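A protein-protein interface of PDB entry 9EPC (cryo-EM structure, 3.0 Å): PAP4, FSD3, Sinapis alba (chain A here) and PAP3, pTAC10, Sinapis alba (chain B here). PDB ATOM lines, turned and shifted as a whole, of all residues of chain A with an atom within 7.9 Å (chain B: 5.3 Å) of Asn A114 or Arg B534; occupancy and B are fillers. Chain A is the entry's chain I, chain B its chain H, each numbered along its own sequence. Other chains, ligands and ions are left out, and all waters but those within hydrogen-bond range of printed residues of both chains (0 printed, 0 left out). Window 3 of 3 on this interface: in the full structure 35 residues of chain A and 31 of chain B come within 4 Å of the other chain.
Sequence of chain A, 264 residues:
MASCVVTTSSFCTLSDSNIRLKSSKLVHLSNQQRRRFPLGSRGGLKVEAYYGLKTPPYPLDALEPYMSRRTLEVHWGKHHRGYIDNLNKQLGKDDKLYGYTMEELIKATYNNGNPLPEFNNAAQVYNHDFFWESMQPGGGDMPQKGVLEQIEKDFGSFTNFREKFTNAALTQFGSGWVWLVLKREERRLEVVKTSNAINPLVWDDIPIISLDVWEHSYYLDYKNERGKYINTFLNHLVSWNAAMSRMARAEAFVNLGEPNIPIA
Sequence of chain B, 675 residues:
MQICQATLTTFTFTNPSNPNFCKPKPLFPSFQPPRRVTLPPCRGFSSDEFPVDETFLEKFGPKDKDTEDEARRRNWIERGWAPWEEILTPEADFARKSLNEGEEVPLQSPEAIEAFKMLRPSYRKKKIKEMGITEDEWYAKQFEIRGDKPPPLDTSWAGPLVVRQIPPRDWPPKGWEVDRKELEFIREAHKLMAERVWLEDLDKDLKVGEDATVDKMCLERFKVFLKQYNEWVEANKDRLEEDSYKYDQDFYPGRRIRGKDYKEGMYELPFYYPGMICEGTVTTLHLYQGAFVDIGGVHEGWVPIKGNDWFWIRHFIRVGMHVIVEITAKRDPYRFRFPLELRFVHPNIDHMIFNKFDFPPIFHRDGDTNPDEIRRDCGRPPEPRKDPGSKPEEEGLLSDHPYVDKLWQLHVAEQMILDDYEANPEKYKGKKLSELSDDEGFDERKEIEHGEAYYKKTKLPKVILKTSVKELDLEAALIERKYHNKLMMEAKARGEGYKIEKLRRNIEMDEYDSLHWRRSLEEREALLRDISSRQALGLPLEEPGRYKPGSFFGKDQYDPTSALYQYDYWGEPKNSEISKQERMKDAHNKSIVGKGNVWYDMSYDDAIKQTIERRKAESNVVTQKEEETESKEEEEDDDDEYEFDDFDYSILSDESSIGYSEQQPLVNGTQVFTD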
ATOM      1  N   ALA A 108       8.976 -40.679   3.940  1.00  0.00           N
ATOM      2  CA  ALA A 108       7.564 -40.732   4.305  1.00  0.00           C
ATOM      3  C   ALA A 108       7.265 -39.814   5.482  1.00  0.00           C
ATOM      4  O   ALA A 108       6.279 -39.068   5.466  1.00  0.00           O
ATOM      5  CB  ALA A 108       7.158 -42.170   4.627  1.00  0.00           C
ATOM      6  N   THR A 109       8.109 -39.850   6.515  1.00  0.00           N
ATOM      7  CA  THR A 109       7.890 -38.988   7.672  1.00  0.00           C
ATOM      8  C   THR A 109       8.118 -37.524   7.332  1.00  0.00           C
ATOM      9  O   THR A 109       7.554 -36.643   7.989  1.00  0.00           O
ATOM     10  CB  THR A 109       8.798 -39.409   8.825  1.00  0.00           C
ATOM     11  OG1 THR A 109      10.139 -39.563   8.345  1.00  0.00           O
ATOM     12  CG2 THR A 109       8.322 -40.719   9.424  1.00  0.00           C
ATOM     13  N   TYR A 110       8.941 -37.243   6.319  1.00  0.00           N
ATOM     14  CA  TYR A 110       9.124 -35.866   5.878  1.00  0.00           C
ATOM     15  C   TYR A 110       7.816 -35.268   5.380  1.00  0.00           C
ATOM     16  O   TYR A 110       7.573 -34.070   5.559  1.00  0.00           O
ATOM     17  CB  TYR A 110      10.195 -35.809   4.792  1.00  0.00           C
ATOM     18  CG  TYR A 110      10.459 -34.427   4.246  1.00  0.00           C
ATOM     19  CD1 TYR A 110      11.036 -33.445   5.036  1.00  0.00           C
ATOM     20  CD2 TYR A 110      10.148 -34.111   2.931  1.00  0.00           C
ATOM     21  CE1 TYR A 110      11.285 -32.184   4.537  1.00  0.00           C
ATOM     22  CE2 TYR A 110      10.398 -32.854   2.422  1.00  0.00           C
ATOM     23  CZ  TYR A 110      10.963 -31.894   3.230  1.00  0.00           C
ATOM     24  OH  TYR A 110      11.209 -30.639   2.727  1.00  0.00           O
ATOM     25  N   ASN A 111       6.969 -36.089   4.758  1.00  0.00           N
ATOM     26  CA  ASN A 111       5.625 -35.690   4.342  1.00  0.00           C
ATOM     27  C   ASN A 111       5.664 -34.471   3.424  1.00  0.00           C
ATOM     28  O   ASN A 111       4.819 -33.578   3.507  1.00  0.00           O
ATOM     29  CB  ASN A 111       4.730 -35.437   5.557  1.00  0.00           C
ATOM     30  CG  ASN A 111       3.261 -35.415   5.200  1.00  0.00           C
ATOM     31  OD1 ASN A 111       2.851 -35.951   4.173  1.00  0.00           O
ATOM     32  ND2 ASN A 111       2.456 -34.791   6.050  1.00  0.00           N
ATOM     33  N   ASN A 112       6.662 -34.438   2.540  1.00  0.00           N
ATOM     34  CA  ASN A 112       6.783 -33.401   1.517  1.00  0.00           C
ATOM     35  C   ASN A 112       6.783 -32.001   2.127  1.00  0.00           C
ATOM     36  O   ASN A 112       6.081 -31.101   1.665  1.00  0.00           O
ATOM     37  CB  ASN A 112       5.678 -33.539   0.468  1.00  0.00           C
ATOM     38  CG  ASN A 112       5.987 -32.780  -0.806  1.00  0.00           C
ATOM     39  OD1 ASN A 112       7.146 -32.499  -1.107  1.00  0.00           O
ATOM     40  ND2 ASN A 112       4.950 -32.445  -1.562  1.00  0.00           N
ATOM     41  N   GLY A 113       7.570 -31.816   3.183  1.00  0.00           N
ATOM     42  CA  GLY A 113       7.755 -30.513   3.782  1.00  0.00           C
ATOM     43  C   GLY A 113       6.956 -30.248   5.036  1.00  0.00           C
ATOM     44  O   GLY A 113       7.060 -29.149   5.593  1.00  0.00           O
ATOM     45  N   ASN A 114       6.167 -31.210   5.502  1.00  0.00           N
ATOM     46  CA  ASN A 114       5.392 -31.081   6.735  1.00  0.00           C
ATOM     47  C   ASN A 114       5.710 -32.282   7.614  1.00  0.00           C
ATOM     48  O   ASN A 114       4.901 -33.208   7.745  1.00  0.00           O
ATOM     49  CB  ASN A 114       3.896 -30.983   6.442  1.00  0.00           C
ATOM     50  CG  ASN A 114       3.074 -30.728   7.686  1.00  0.00           C
ATOM     51  OD1 ASN A 114       3.604 -30.323   8.721  1.00  0.00           O
ATOM     52  ND2 ASN A 114       1.771 -30.963   7.593  1.00  0.00           N
ATOM     53  N   PRO A 115       6.888 -32.292   8.237  1.00  0.00           N
ATOM     54  CA  PRO A 115       7.370 -33.511   8.894  1.00  0.00           C
ATOM     55  C   PRO A 115       6.430 -33.999   9.987  1.00  0.00           C
ATOM     56  O   PRO A 115       5.843 -33.211  10.732  1.00  0.00           O
ATOM     57  CB  PRO A 115       8.724 -33.085   9.473  1.00  0.00           C
ATOM     58  CG  PRO A 115       9.135 -31.910   8.653  1.00  0.00           C
ATOM     59  CD  PRO A 115       7.865 -31.196   8.317  1.00  0.00           C
ATOM     60  N   LEU A 116       6.291 -35.318  10.064  1.00  0.00           N
ATOM     61  CA  LEU A 116       5.530 -35.948  11.122  1.00  0.00           C
ATOM     62  C   LEU A 116       6.313 -35.883  12.431  1.00  0.00           C
ATOM     63  O   LEU A 116       7.520 -35.629  12.428  1.00  0.00           O
ATOM     64  CB  LEU A 116       5.220 -37.396  10.752  1.00  0.00           C
ATOM     65  CG  LEU A 116       4.544 -37.600   9.396  1.00  0.00           C
ATOM     66  CD1 LEU A 116       4.216 -39.064   9.175  1.00  0.00           C
ATOM     67  CD2 LEU A 116       3.296 -36.743   9.287  1.00  0.00           C
ATOM     68  N   PRO A 117       5.645 -36.090  13.570  1.00  0.00           N
ATOM     69  CA  PRO A 117       6.373 -36.053  14.849  1.00  0.00           C
ATOM     70  C   PRO A 117       7.499 -37.067  14.932  1.00  0.00           C
ATOM     71  O   PRO A 117       8.457 -36.854  15.684  1.00  0.00           O
ATOM     72  CB  PRO A 117       5.276 -36.345  15.882  1.00  0.00           C
ATOM     73  CG  PRO A 117       4.022 -35.893  15.227  1.00  0.00           C
ATOM     74  CD  PRO A 117       4.190 -36.210  13.772  1.00  0.00           C
ATOM     75  N   PHE A 119       9.505 -37.767  12.459  1.00  0.00           N
ATOM     76  CA  PHE A 119      10.554 -37.453  11.494  1.00  0.00           C
ATOM     77  C   PHE A 119      11.853 -37.052  12.180  1.00  0.00           C
ATOM     78  O   PHE A 119      12.935 -37.476  11.761  1.00  0.00           O
ATOM     79  CB  PHE A 119      10.092 -36.344  10.552  1.00  0.00           C
ATOM     80  CG  PHE A 119      11.173 -35.834   9.646  1.00  0.00           C
ATOM     81  CD1 PHE A 119      11.509 -36.523   8.494  1.00  0.00           C
ATOM     82  CD2 PHE A 119      11.855 -34.669   9.945  1.00  0.00           C
ATOM     83  CE1 PHE A 119      12.502 -36.059   7.660  1.00  0.00           C
ATOM     84  CE2 PHE A 119      12.851 -34.201   9.114  1.00  0.00           C
ATOM     85  CZ  PHE A 119      13.175 -34.897   7.970  1.00  0.00           C
ATOM     86  N   SER A 195      19.255 -27.532   7.900  1.00  0.00           N
ATOM     87  CA  SER A 195      19.158 -27.225   9.317  1.00  0.00           C
ATOM     88  C   SER A 195      18.425 -28.332  10.065  1.00  0.00           C
ATOM     89  O   SER A 195      17.565 -29.023   9.511  1.00  0.00           O
ATOM     90  CB  SER A 195      18.440 -25.894   9.526  1.00  0.00           C
ATOM     91  OG  SER A 195      17.151 -25.920   8.940  1.00  0.00           O
ATOM     92  N   ASP B 530       4.233 -20.124  11.781  1.00  0.00           N
ATOM     93  CA  ASP B 530       4.693 -21.222  10.942  1.00  0.00           C
ATOM     94  C   ASP B 530       5.591 -20.729   9.815  1.00  0.00           C
ATOM     95  O   ASP B 530       6.477 -21.464   9.367  1.00  0.00           O
ATOM     96  CB  ASP B 530       3.494 -21.980  10.373  1.00  0.00           C
ATOM     97  CG  ASP B 530       3.876 -23.328   9.798  1.00  0.00           C
ATOM     98  OD1 ASP B 530       5.007 -23.788  10.058  1.00  0.00           O
ATOM     99  OD2 ASP B 530       3.047 -23.930   9.085  1.00  0.00           O
ATOM    100  N   ILE B 531       5.379 -19.498   9.345  1.00  0.00           N
ATOM    101  CA  ILE B 531       6.150 -18.990   8.213  1.00  0.00           C
ATOM    102  C   ILE B 531       7.624 -18.866   8.579  1.00  0.00           C
ATOM    103  O   ILE B 531       8.501 -19.370   7.869  1.00  0.00           O
ATOM    104  CB  ILE B 531       5.577 -17.647   7.730  1.00  0.00           C
ATOM    105  CG1 ILE B 531       4.235 -17.860   7.034  1.00  0.00           C
ATOM    106  CG2 ILE B 531       6.559 -16.952   6.803  1.00  0.00           C
ATOM    107  CD1 ILE B 531       3.589 -16.583   6.559  1.00  0.00           C
ATOM    108  N   SER B 532       7.916 -18.203   9.699  1.00  0.00           N
ATOM    109  CA  SER B 532       9.309 -17.969  10.070  1.00  0.00           C
ATOM    110  C   SER B 532      10.029 -19.273  10.374  1.00  0.00           C
ATOM    111  O   SER B 532      11.189 -19.451   9.985  1.00  0.00           O
ATOM    112  CB  SER B 532       9.391 -17.038  11.272  1.00  0.00           C
ATOM    113  OG  SER B 532       9.057 -17.735  12.459  1.00  0.00           O
ATOM    114  N   SER B 533       9.361 -20.192  11.075  1.00  0.00           N
ATOM    115  CA  SER B 533       9.989 -21.466  11.402  1.00  0.00           C
ATOM    116  C   SER B 533      10.401 -22.207  10.140  1.00  0.00           C
ATOM    117  O   SER B 533      11.495 -22.777  10.076  1.00  0.00           O
ATOM    118  CB  SER B 533       9.041 -22.317  12.243  1.00  0.00           C
ATOM    119  OG  SER B 533       8.709 -21.659  13.451  1.00  0.00           O
ATOM    120  N   ARG B 534       9.542 -22.200   9.122  1.00  0.00           N
ATOM    121  CA  ARG B 534       9.919 -22.787   7.843  1.00  0.00           C
ATOM    122  C   ARG B 534      10.935 -21.918   7.115  1.00  0.00           C
ATOM    123  O   ARG B 534      11.856 -22.437   6.474  1.00  0.00           O
ATOM    124  CB  ARG B 534       8.674 -23.004   6.987  1.00  0.00           C
ATOM    125  CG  ARG B 534       7.681 -23.956   7.617  1.00  0.00           C
ATOM    126  CD  ARG B 534       6.464 -24.159   6.744  1.00  0.00           C
ATOM    127  NE  ARG B 534       5.579 -25.172   7.306  1.00  0.00           N
ATOM    128  CZ  ARG B 534       5.692 -26.471   7.072  1.00  0.00           C
ATOM    129  NH1 ARG B 534       6.636 -26.950   6.281  1.00  0.00           N
ATOM    130  NH2 ARG B 534       4.837 -27.309   7.648  1.00  0.00           N
ATOM    131  N   GLN B 535      10.784 -20.594   7.199  1.00  0.00           N
ATOM    132  CA  GLN B 535      11.750 -19.701   6.568  1.00  0.00           C
ATOM    133  C   GLN B 535      13.127 -19.838   7.203  1.00  0.00           C
ATOM    134  O   GLN B 535      14.141 -19.898   6.498  1.00  0.00           O
ATOM    135  CB  GLN B 535      11.268 -18.253   6.656  1.00  0.00           C
ATOM    136  CG  GLN B 535      10.223 -17.887   5.624  1.00  0.00           C
ATOM    137  CD  GLN B 535      10.763 -17.951   4.212  1.00  0.00           C
ATOM    138  OE1 GLN B 535      10.664 -18.977   3.542  1.00  0.00           O
ATOM    139  NE2 GLN B 535      11.341 -16.848   3.751  1.00  0.00           N
ATOM    140  N   ALA B 536      13.186 -19.893   8.534  1.00  0.00           N
ATOM    141  CA  ALA B 536      14.470 -20.016   9.211  1.00  0.00           C
ATOM    142  C   ALA B 536      15.073 -21.404   9.061  1.00  0.00           C
ATOM    143  O   ALA B 536      16.276 -21.570   9.283  1.00  0.00           O
ATOM    144  CB  ALA B 536      14.322 -19.671  10.693  1.00  0.00           C
ATOM    145  N   LEU B 537      14.271 -22.401   8.694  1.00  0.00           N
ATOM    146  CA  LEU B 537      14.744 -23.768   8.549  1.00  0.00           C
ATOM    147  C   LEU B 537      14.793 -24.230   7.100  1.00  0.00           C
ATOM    148  O   LEU B 537      15.221 -25.358   6.839  1.00  0.00           O
ATOM    149  CB  LEU B 537      13.862 -24.724   9.359  1.00  0.00           C
ATOM    150  CG  LEU B 537      14.164 -24.936  10.844  1.00  0.00           C
ATOM    151  CD1 LEU B 537      14.272 -23.628  11.598  1.00  0.00           C
ATOM    152  CD2 LEU B 537      13.083 -25.803  11.455  1.00  0.00           C
ATOM    153  N   GLY B 538      14.365 -23.398   6.157  1.00  0.00           N
ATOM    154  CA  GLY B 538      14.348 -23.778   4.762  1.00  0.00           C
ATOM    155  C   GLY B 538      13.168 -24.621   4.343  1.00  0.00           C
ATOM    156  O   GLY B 538      13.088 -25.001   3.168  1.00  0.00           O
ATOM    157  N   LEU B 539      12.252 -24.929   5.257  1.00  0.00           N
ATOM    158  CA  LEU B 539      11.082 -25.709   4.900  1.00  0.00           C
ATOM    159  C   LEU B 539      10.178 -24.907   3.965  1.00  0.00           C
ATOM    160  O   LEU B 539      10.046 -23.689   4.107  1.00  0.00           O
ATOM    161  CB  LEU B 539      10.311 -26.115   6.152  1.00  0.00           C
ATOM    162  CG  LEU B 539      11.104 -26.943   7.162  1.00  0.00           C
ATOM    163  CD1 LEU B 539      10.247 -27.280   8.369  1.00  0.00           C
ATOM    164  CD2 LEU B 539      11.633 -28.206   6.510  1.00  0.00           C
ATOM    165  N   PRO B 540       9.555 -25.568   2.991  1.00  0.00           N
ATOM    166  CA  PRO B 540       8.707 -24.842   2.039  1.00  0.00           C
ATOM    167  C   PRO B 540       7.491 -24.236   2.718  1.00  0.00           C
ATOM    168  O   PRO B 540       6.842 -24.869   3.555  1.00  0.00           O
ATOM    169  CB  PRO B 540       8.303 -25.924   1.033  1.00  0.00           C
ATOM    170  CG  PRO B 540       8.406 -27.198   1.801  1.00  0.00           C
ATOM    171  CD  PRO B 540       9.564 -27.017   2.732  1.00  0.00           C
ATOM    172  N   LEU B 541       7.183 -22.993   2.345  1.00  0.00           N
ATOM    173  CA  LEU B 541       6.000 -22.334   2.888  1.00  0.00           C
ATOM    174  C   LEU B 541       4.726 -22.931   2.309  1.00  0.00           C
ATOM    175  O   LEU B 541       3.752 -23.156   3.037  1.00  0.00           O
ATOM    176  CB  LEU B 541       6.063 -20.834   2.614  1.00  0.00           C
ATOM    177  CG  LEU B 541       7.264 -20.106   3.212  1.00  0.00           C
ATOM    178  CD1 LEU B 541       7.202 -18.623   2.894  1.00  0.00           C
ATOM    179  CD2 LEU B 541       7.329 -20.334   4.712  1.00  0.00           C
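Asn A114 touches just one residue of chain B: Arg B534 (3.4 Å). Arg B534 touches just these residues of chain A: Gly A113 (2.3 Å) and Asn A114 (3.4 Å). Of the printed residues of chain A, Leu B537 touches Ser A195 (2.9 Å). Of the printed residues of chain B, Tyr A110 touches Pro B540 (3.98 Å). Pro A115 touches none of the printed residues of chain B. Ala B536 touches none of the printed residues of chain A.
OH of Tyr A110 touches CD of Pro B540 (3.98 Å). CA of Gly A113 touches CG of Pro B540, 3.9 Å away.
OD1 of Asp B530 is in salt-bridge range of NE of Arg B534, 3.1 Å away. The backbone carbonyl oxygen of Arg B534 is in hydrogen-bond range of the backbone NH of Leu B539, 2.8 Å away. The guanidinium group (NH1) of Arg B534 lies close to the backbone carbonyl oxygen (O) of Pro B540, 3.4 Å away. The side-chain amide nitrogen (ND2) of Asn A111 lies close to the backbone carbonyl oxygen (O) of Asn A114.
NH2 of Arg B534 lies within hydrogen-bond range of OD1 of Asn A114. The side-chain hydroxyl (OG) of Ser A195 lies within hydrogen-bond range of the backbone carbonyl oxygen (O) of Leu B537 (2.9 Å). The backbone carbonyl oxygen (O) of Gly A113 sits close to the guanidinium group (NH1) of Arg B534.
Of the 12 printed residues of chain A, 4 touch a printed residue of chain B. Printed residues of chain A that touch a printed residue of chain B: Tyr A110, Gly A113, Asn A114 and Ser A195. Hydrophobic or aromatic side chains of chain A that line the printed part of chain B: Tyr A110. Along chain A the printed residues that touch a printed residue of chain B span positions 110 to 195. Printed residues of chain B that touch a printed residue of chain A: Arg B534, Leu B537 and Pro B540. Hydrophobic or aromatic side chains of chain B that line the printed part of chain A: Leu B537 and Pro B540. Among the printed residues, no Asp or Glu carboxylate lies within 4 Å of a Lys or Arg side-chain nitrogen of the other chain.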
